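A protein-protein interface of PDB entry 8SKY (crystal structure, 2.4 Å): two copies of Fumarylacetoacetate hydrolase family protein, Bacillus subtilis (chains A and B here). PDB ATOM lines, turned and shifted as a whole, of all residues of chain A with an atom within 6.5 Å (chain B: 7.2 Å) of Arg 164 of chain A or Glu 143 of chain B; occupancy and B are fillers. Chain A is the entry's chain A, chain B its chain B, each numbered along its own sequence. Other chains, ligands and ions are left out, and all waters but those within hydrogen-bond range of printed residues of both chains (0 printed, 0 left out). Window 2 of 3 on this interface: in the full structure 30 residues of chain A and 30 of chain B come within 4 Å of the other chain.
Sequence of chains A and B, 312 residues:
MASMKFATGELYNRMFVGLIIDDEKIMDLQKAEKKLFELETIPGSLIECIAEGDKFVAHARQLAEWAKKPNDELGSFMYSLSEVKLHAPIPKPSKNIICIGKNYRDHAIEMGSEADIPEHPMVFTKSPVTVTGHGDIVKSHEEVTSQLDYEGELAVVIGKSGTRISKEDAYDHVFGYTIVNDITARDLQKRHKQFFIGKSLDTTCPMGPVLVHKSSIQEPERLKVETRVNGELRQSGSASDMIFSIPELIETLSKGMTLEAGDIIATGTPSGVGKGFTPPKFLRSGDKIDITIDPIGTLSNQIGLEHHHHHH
NZ of Lys 255 of chain A lies close to NH2 of Arg 191 of chain B, 3.0 Å away.
No position is printed for both chains.
Of the 4 pairs that touch across the chains among the printed residues, none has its exchanged pair printed and touching as well.
O of Ser 254 of chain A is in hydrogen-bond range of N of Arg 164 of chain A (2.7 Å).
Of the 11 printed residues of chain B, 4 touch a printed residue of chain A.
Printed residues of chain B that touch a printed residue of chain A: His 141, Glu 143, Val 144 and Arg 191.
Hydrophobic or aromatic side chains of chain B within 4 Å of the printed part of chain A: His 141 and Val 144.
Among the printed residues, 4 pairs touch across the chains.
Of the printed residues of chain B, Arg 164 of chain A touches Glu 143.
Ser 166 of chain A touches none of the printed residues of chain B.
Of the printed residues of chain B, Lys 255 of chain A touches Val 144 and Arg 191.
Of the printed residues of chain B, Gly 256 of chain A touches His 141.
Ser 140 of chain B touches none of the printed residues of chain A.
Of the printed residues of chain A, His 141 of chain B touches Gly 256.
Printed residues of chain A within 4 Å of Glu 143 of chain B: Arg 164 (3.98 Å).
Of the printed residues of chain A, Val 144 of chain B touches Lys 255.
Of the printed residues of chain A, Arg 191 of chain B touches Lys 255 (3.0 Å).
The nearest printed residue of chain B that does not touch Arg 164 of chain A is Val 144 of chain B (5.5 Å).
The nearest printed residue of chain A that does not touch Arg 191 of chain B is Gly 256 of chain A (8.9 Å).
Glu 143 of chain B touches Arg 164 of chain A.
Lys 255 of chain A touches Val 144 of chain B.
CE1 of His 141 of chain B touches O of Gly 256 of chain A, 3.1 Å away.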
ATOM      1  N   GLY A 162      -4.657  35.955  24.298  1.00  0.00           N
ATOM      2  CA  GLY A 162      -5.008  34.942  25.272  1.00  0.00           C
ATOM      3  C   GLY A 162      -5.551  33.705  24.590  1.00  0.00           C
ATOM      4  O   GLY A 162      -6.006  33.746  23.441  1.00  0.00           O
ATOM      5  N   THR A 163      -5.475  32.598  25.320  1.00  0.00           N
ATOM      6  CA  THR A 163      -6.127  31.353  24.948  1.00  0.00           C
ATOM      7  C   THR A 163      -6.850  30.814  26.174  1.00  0.00           C
ATOM      8  O   THR A 163      -6.498  31.135  27.314  1.00  0.00           O
ATOM      9  CB  THR A 163      -5.129  30.316  24.406  1.00  0.00           C
ATOM     10  OG1 THR A 163      -5.839  29.277  23.719  1.00  0.00           O
ATOM     11  CG2 THR A 163      -4.315  29.705  25.537  1.00  0.00           C
ATOM     12  N   ARG A 164      -7.882  30.008  25.928  1.00  0.00           N
ATOM     13  CA  ARG A 164      -8.725  29.466  26.995  1.00  0.00           C
ATOM     14  C   ARG A 164      -9.307  30.593  27.849  1.00  0.00           C
ATOM     15  O   ARG A 164      -9.176  30.612  29.076  1.00  0.00           O
ATOM     16  CB  ARG A 164      -7.952  28.463  27.852  1.00  0.00           C
ATOM     17  CG  ARG A 164      -8.185  27.019  27.455  1.00  0.00           C
ATOM     18  CD  ARG A 164      -7.490  26.064  28.414  1.00  0.00           C
ATOM     19  NE  ARG A 164      -8.258  25.819  29.634  1.00  0.00           N
ATOM     20  CZ  ARG A 164      -9.460  25.248  29.684  1.00  0.00           C
ATOM     21  NH1 ARG A 164     -10.064  24.833  28.577  1.00  0.00           N
ATOM     22  NH2 ARG A 164     -10.058  25.081  30.854  1.00  0.00           N
ATOM     23  N   ILE A 165      -9.944  31.545  27.180  1.00  0.00           N
ATOM     24  CA  ILE A 165     -10.548  32.699  27.832  1.00  0.00           C
ATOM     25  C   ILE A 165     -11.965  32.336  28.252  1.00  0.00           C
ATOM     26  O   ILE A 165     -12.746  31.814  27.447  1.00  0.00           O
ATOM     27  CB  ILE A 165     -10.546  33.915  26.893  1.00  0.00           C
ATOM     28  CG1 ILE A 165      -9.171  34.070  26.238  1.00  0.00           C
ATOM     29  CG2 ILE A 165     -10.952  35.179  27.641  1.00  0.00           C
ATOM     30  CD1 ILE A 165      -9.040  35.299  25.374  1.00  0.00           C
ATOM     31  N   SER A 166     -12.298  32.597  29.513  1.00  0.00           N
ATOM     32  CA  SER A 166     -13.665  32.386  29.956  1.00  0.00           C
ATOM     33  C   SER A 166     -14.554  33.520  29.459  1.00  0.00           C
ATOM     34  O   SER A 166     -14.088  34.624  29.166  1.00  0.00           O
ATOM     35  CB  SER A 166     -13.741  32.293  31.482  1.00  0.00           C
ATOM     36  OG  SER A 166     -13.357  33.513  32.095  1.00  0.00           O
ATOM     37  N   ASP A 169     -14.058  36.566  31.491  1.00  0.00           N
ATOM     38  CA  ASP A 169     -12.903  37.407  31.199  1.00  0.00           C
ATOM     39  C   ASP A 169     -12.898  37.952  29.776  1.00  0.00           C
ATOM     40  O   ASP A 169     -11.956  38.660  29.408  1.00  0.00           O
ATOM     41  CB  ASP A 169     -11.604  36.626  31.433  1.00  0.00           C
ATOM     42  CG  ASP A 169     -11.413  36.220  32.879  1.00  0.00           C
ATOM     43  OD1 ASP A 169     -11.799  37.000  33.774  1.00  0.00           O
ATOM     44  OD2 ASP A 169     -10.869  35.121  33.116  1.00  0.00           O
ATOM     45  N   GLU A 251     -15.008  32.936  24.155  1.00  0.00           N
ATOM     46  CA  GLU A 251     -14.752  31.701  24.889  1.00  0.00           C
ATOM     47  C   GLU A 251     -14.677  30.509  23.944  1.00  0.00           C
ATOM     48  O   GLU A 251     -13.804  29.644  24.090  1.00  0.00           O
ATOM     49  CB  GLU A 251     -15.834  31.484  25.947  1.00  0.00           C
ATOM     50  CG  GLU A 251     -15.700  30.174  26.711  1.00  0.00           C
ATOM     51  CD  GLU A 251     -17.001  29.726  27.352  1.00  0.00           C
ATOM     52  OE1 GLU A 251     -17.903  29.270  26.617  1.00  0.00           O
ATOM     53  OE2 GLU A 251     -17.120  29.826  28.591  1.00  0.00           O
ATOM     54  N   SER A 254     -11.489  30.673  21.455  1.00  0.00           N
ATOM     55  CA  SER A 254     -10.189  30.563  22.102  1.00  0.00           C
ATOM     56  C   SER A 254     -10.022  29.286  22.915  1.00  0.00           C
ATOM     57  O   SER A 254      -9.057  29.182  23.679  1.00  0.00           O
ATOM     58  CB  SER A 254      -9.946  31.778  22.998  1.00  0.00           C
ATOM     59  OG  SER A 254     -10.590  31.621  24.249  1.00  0.00           O
ATOM     60  N   LYS A 255     -10.929  28.312  22.775  1.00  0.00           N
ATOM     61  CA  LYS A 255     -10.829  27.112  23.604  1.00  0.00           C
ATOM     62  C   LYS A 255      -9.527  26.363  23.338  1.00  0.00           C
ATOM     63  O   LYS A 255      -8.861  25.913  24.278  1.00  0.00           O
ATOM     64  CB  LYS A 255     -12.039  26.197  23.384  1.00  0.00           C
ATOM     65  CG  LYS A 255     -12.365  25.848  21.941  1.00  0.00           C
ATOM     66  CD  LYS A 255     -13.670  25.065  21.867  1.00  0.00           C
ATOM     67  CE  LYS A 255     -14.106  24.831  20.432  1.00  0.00           C
ATOM     68  NZ  LYS A 255     -15.394  24.086  20.369  1.00  0.00           N
ATOM     69  N   GLY A 256      -9.139  26.237  22.071  1.00  0.00           N
ATOM     70  CA  GLY A 256      -7.878  25.609  21.727  1.00  0.00           C
ATOM     71  C   GLY A 256      -7.093  26.414  20.711  1.00  0.00           C
ATOM     72  O   GLY A 256      -6.343  25.854  19.904  1.00  0.00           O
ATOM     73  N   MET A 257      -7.251  27.735  20.751  1.00  0.00           N
ATOM     74  CA  MET A 257      -6.655  28.613  19.756  1.00  0.00           C
ATOM     75  C   MET A 257      -6.385  29.966  20.396  1.00  0.00           C
ATOM     76  O   MET A 257      -7.221  30.482  21.142  1.00  0.00           O
ATOM     77  CB  MET A 257      -7.578  28.758  18.538  1.00  0.00           C
ATOM     78  CG  MET A 257      -7.221  29.889  17.591  1.00  0.00           C
ATOM     79  SD  MET A 257      -8.273  29.897  16.125  1.00  0.00           S
ATOM     80  CE  MET A 257      -9.620  30.942  16.676  1.00  0.00           C
ATOM     81  N   THR A 258      -5.218  30.533  20.109  1.00  0.00           N
ATOM     82  CA  THR A 258      -4.832  31.811  20.684  1.00  0.00           C
ATOM     83  C   THR A 258      -5.396  32.955  19.853  1.00  0.00           C
ATOM     84  O   THR A 258      -5.167  33.027  18.640  1.00  0.00           O
ATOM     85  CB  THR A 258      -3.309  31.940  20.779  1.00  0.00           C
ATOM     86  OG1 THR A 258      -2.795  30.929  21.654  1.00  0.00           O
ATOM     87  CG2 THR A 258      -2.926  33.313  21.321  1.00  0.00           C
ATOM     88  N   LYS B 139       0.668  20.339  20.217  1.00  0.00           N
ATOM     89  CA  LYS B 139      -0.207  20.218  21.374  1.00  0.00           C
ATOM     90  C   LYS B 139      -1.318  19.210  21.107  1.00  0.00           C
ATOM     91  O   LYS B 139      -1.881  19.155  20.012  1.00  0.00           O
ATOM     92  CB  LYS B 139      -0.814  21.577  21.728  1.00  0.00           C
ATOM     93  CG  LYS B 139       0.092  22.483  22.539  1.00  0.00           C
ATOM     94  CD  LYS B 139      -0.480  23.888  22.604  1.00  0.00           C
ATOM     95  CE  LYS B 139       0.429  24.830  23.373  1.00  0.00           C
ATOM     96  NZ  LYS B 139       0.007  26.249  23.213  1.00  0.00           N
ATOM     97  N   SER B 140      -1.631  18.406  22.126  1.00  0.00           N
ATOM     98  CA  SER B 140      -2.696  17.422  21.981  1.00  0.00           C
ATOM     99  C   SER B 140      -4.073  18.073  21.995  1.00  0.00           C
ATOM    100  O   SER B 140      -4.988  17.590  21.316  1.00  0.00           O
ATOM    101  CB  SER B 140      -2.599  16.370  23.087  1.00  0.00           C
ATOM    102  OG  SER B 140      -2.658  16.970  24.369  1.00  0.00           O
ATOM    103  N   HIS B 141      -4.238  19.163  22.751  1.00  0.00           N
ATOM    104  CA  HIS B 141      -5.530  19.837  22.900  1.00  0.00           C
ATOM    105  C   HIS B 141      -6.599  18.869  23.403  1.00  0.00           C
ATOM    106  O   HIS B 141      -7.740  18.881  22.935  1.00  0.00           O
ATOM    107  CB  HIS B 141      -5.977  20.488  21.587  1.00  0.00           C
ATOM    108  CG  HIS B 141      -5.140  21.656  21.165  1.00  0.00           C
ATOM    109  ND1 HIS B 141      -5.286  22.915  21.710  1.00  0.00           N
ATOM    110  CD2 HIS B 141      -4.157  21.760  20.239  1.00  0.00           C
ATOM    111  CE1 HIS B 141      -4.426  23.740  21.141  1.00  0.00           C
ATOM    112  NE2 HIS B 141      -3.729  23.063  20.246  1.00  0.00           N
ATOM    113  N   GLU B 142      -6.228  18.015  24.363  1.00  0.00           N
ATOM    114  CA  GLU B 142      -7.133  16.944  24.776  1.00  0.00           C
ATOM    115  C   GLU B 142      -8.385  17.481  25.460  1.00  0.00           C
ATOM    116  O   GLU B 142      -9.449  16.859  25.372  1.00  0.00           O
ATOM    117  CB  GLU B 142      -6.421  15.955  25.698  1.00  0.00           C
ATOM    118  CG  GLU B 142      -7.202  14.659  25.875  1.00  0.00           C
ATOM    119  CD  GLU B 142      -6.915  13.955  27.185  1.00  0.00           C
ATOM    120  OE1 GLU B 142      -7.730  14.091  28.121  1.00  0.00           O
ATOM    121  OE2 GLU B 142      -5.886  13.253  27.274  1.00  0.00           O
ATOM    122  N   GLU B 143      -8.287  18.623  26.132  1.00  0.00           N
ATOM    123  CA  GLU B 143      -9.464  19.218  26.765  1.00  0.00           C
ATOM    124  C   GLU B 143     -10.442  19.817  25.755  1.00  0.00           C
ATOM    125  O   GLU B 143     -11.440  20.432  26.158  1.00  0.00           O
ATOM    126  CB  GLU B 143      -9.036  20.289  27.769  1.00  0.00           C
ATOM    127  CG  GLU B 143      -8.400  21.513  27.133  1.00  0.00           C
ATOM    128  CD  GLU B 143      -6.929  21.313  26.827  1.00  0.00           C
ATOM    129  OE1 GLU B 143      -6.279  20.521  27.540  1.00  0.00           O
ATOM    130  OE2 GLU B 143      -6.424  21.944  25.874  1.00  0.00           O
ATOM    131  N   VAL B 144     -10.170  19.662  24.461  1.00  0.00           N
ATOM    132  CA  VAL B 144     -11.021  20.206  23.410  1.00  0.00           C
ATOM    133  C   VAL B 144     -11.465  19.085  22.478  1.00  0.00           C
ATOM    134  O   VAL B 144     -12.640  18.999  22.103  1.00  0.00           O
ATOM    135  CB  VAL B 144     -10.293  21.323  22.642  1.00  0.00           C
ATOM    136  CG1 VAL B 144     -11.054  21.691  21.387  1.00  0.00           C
ATOM    137  CG2 VAL B 144     -10.112  22.537  23.536  1.00  0.00           C
ATOM    138  N   THR B 145     -10.525  18.224  22.092  1.00  0.00           N
ATOM    139  CA  THR B 145     -10.794  17.157  21.139  1.00  0.00           C
ATOM    140  C   THR B 145     -10.151  15.861  21.610  1.00  0.00           C
ATOM    141  O   THR B 145      -9.202  15.858  22.398  1.00  0.00           O
ATOM    142  CB  THR B 145     -10.272  17.508  19.737  1.00  0.00           C
ATOM    143  OG1 THR B 145     -10.660  16.487  18.808  1.00  0.00           O
ATOM    144  CG2 THR B 145      -8.754  17.625  19.747  1.00  0.00           C
ATOM    145  N   SER B 146     -10.705  14.751  21.122  1.00  0.00           N
ATOM    146  CA  SER B 146     -10.068  13.443  21.213  1.00  0.00           C
ATOM    147  C   SER B 146     -10.011  12.775  19.847  1.00  0.00           C
ATOM    148  O   SER B 146      -9.658  11.593  19.755  1.00  0.00           O
ATOM    149  CB  SER B 146     -10.798  12.545  22.218  1.00  0.00           C
ATOM    150  OG  SER B 146     -10.721  13.083  23.525  1.00  0.00           O
ATOM    151  N   ARG B 191     -18.697  19.522  14.496  1.00  0.00           N
ATOM    152  CA  ARG B 191     -19.514  20.341  15.390  1.00  0.00           C
ATOM    153  C   ARG B 191     -19.802  21.713  14.789  1.00  0.00           C
ATOM    154  O   ARG B 191     -20.947  22.180  14.797  1.00  0.00           O
ATOM    155  CB  ARG B 191     -18.845  20.502  16.758  1.00  0.00           C
ATOM    156  CG  ARG B 191     -19.395  21.725  17.493  1.00  0.00           C
ATOM    157  CD  ARG B 191     -19.399  21.661  19.017  1.00  0.00           C
ATOM    158  NE  ARG B 191     -18.084  21.593  19.647  1.00  0.00           N
ATOM    159  CZ  ARG B 191     -17.904  21.621  20.964  1.00  0.00           C
ATOM    160  NH1 ARG B 191     -18.952  21.730  21.774  1.00  0.00           N
ATOM    161  NH2 ARG B 191     -16.683  21.558  21.473  1.00  0.00           N
ATOM    162  N   LEU B 305       2.054  16.001  25.539  1.00  0.00           N
ATOM    163  CA  LEU B 305       1.311  15.543  26.701  1.00  0.00           C
ATOM    164  C   LEU B 305       0.203  16.500  27.097  1.00  0.00           C
ATOM    165  O   LEU B 305       0.251  17.686  26.769  1.00  0.00           O
ATOM    166  CB  LEU B 305       2.249  15.304  27.888  1.00  0.00           C
ATOM    167  CG  LEU B 305       2.673  13.856  28.152  1.00  0.00           C
ATOM    168  CD1 LEU B 305       1.460  12.990  28.454  1.00  0.00           C
ATOM    169  CD2 LEU B 305       3.475  13.278  26.996  1.00  0.00           C
ATOM    170  N   GLU B 306      -0.793  15.989  27.803  1.00  0.00           N
ATOM    171  CA  GLU B 306      -1.918  16.798  28.248  1.00  0.00           C
ATOM    172  C   GLU B 306      -1.570  17.607  29.486  1.00  0.00           C
ATOM    173  O   GLU B 306      -2.085  18.692  29.694  1.00  0.00           O
ATOM    174  CB  GLU B 306      -3.051  15.863  28.622  1.00  0.00           C
ATOM    175  CG  GLU B 306      -2.612  14.699  29.496  1.00  0.00           C
ATOM    176  CD  GLU B 306      -3.746  13.757  29.856  1.00  0.00           C
ATOM    177  OE1 GLU B 306      -4.891  14.224  30.028  1.00  0.00           O
ATOM    178  OE2 GLU B 306      -3.489  12.545  29.979  1.00  0.00           O
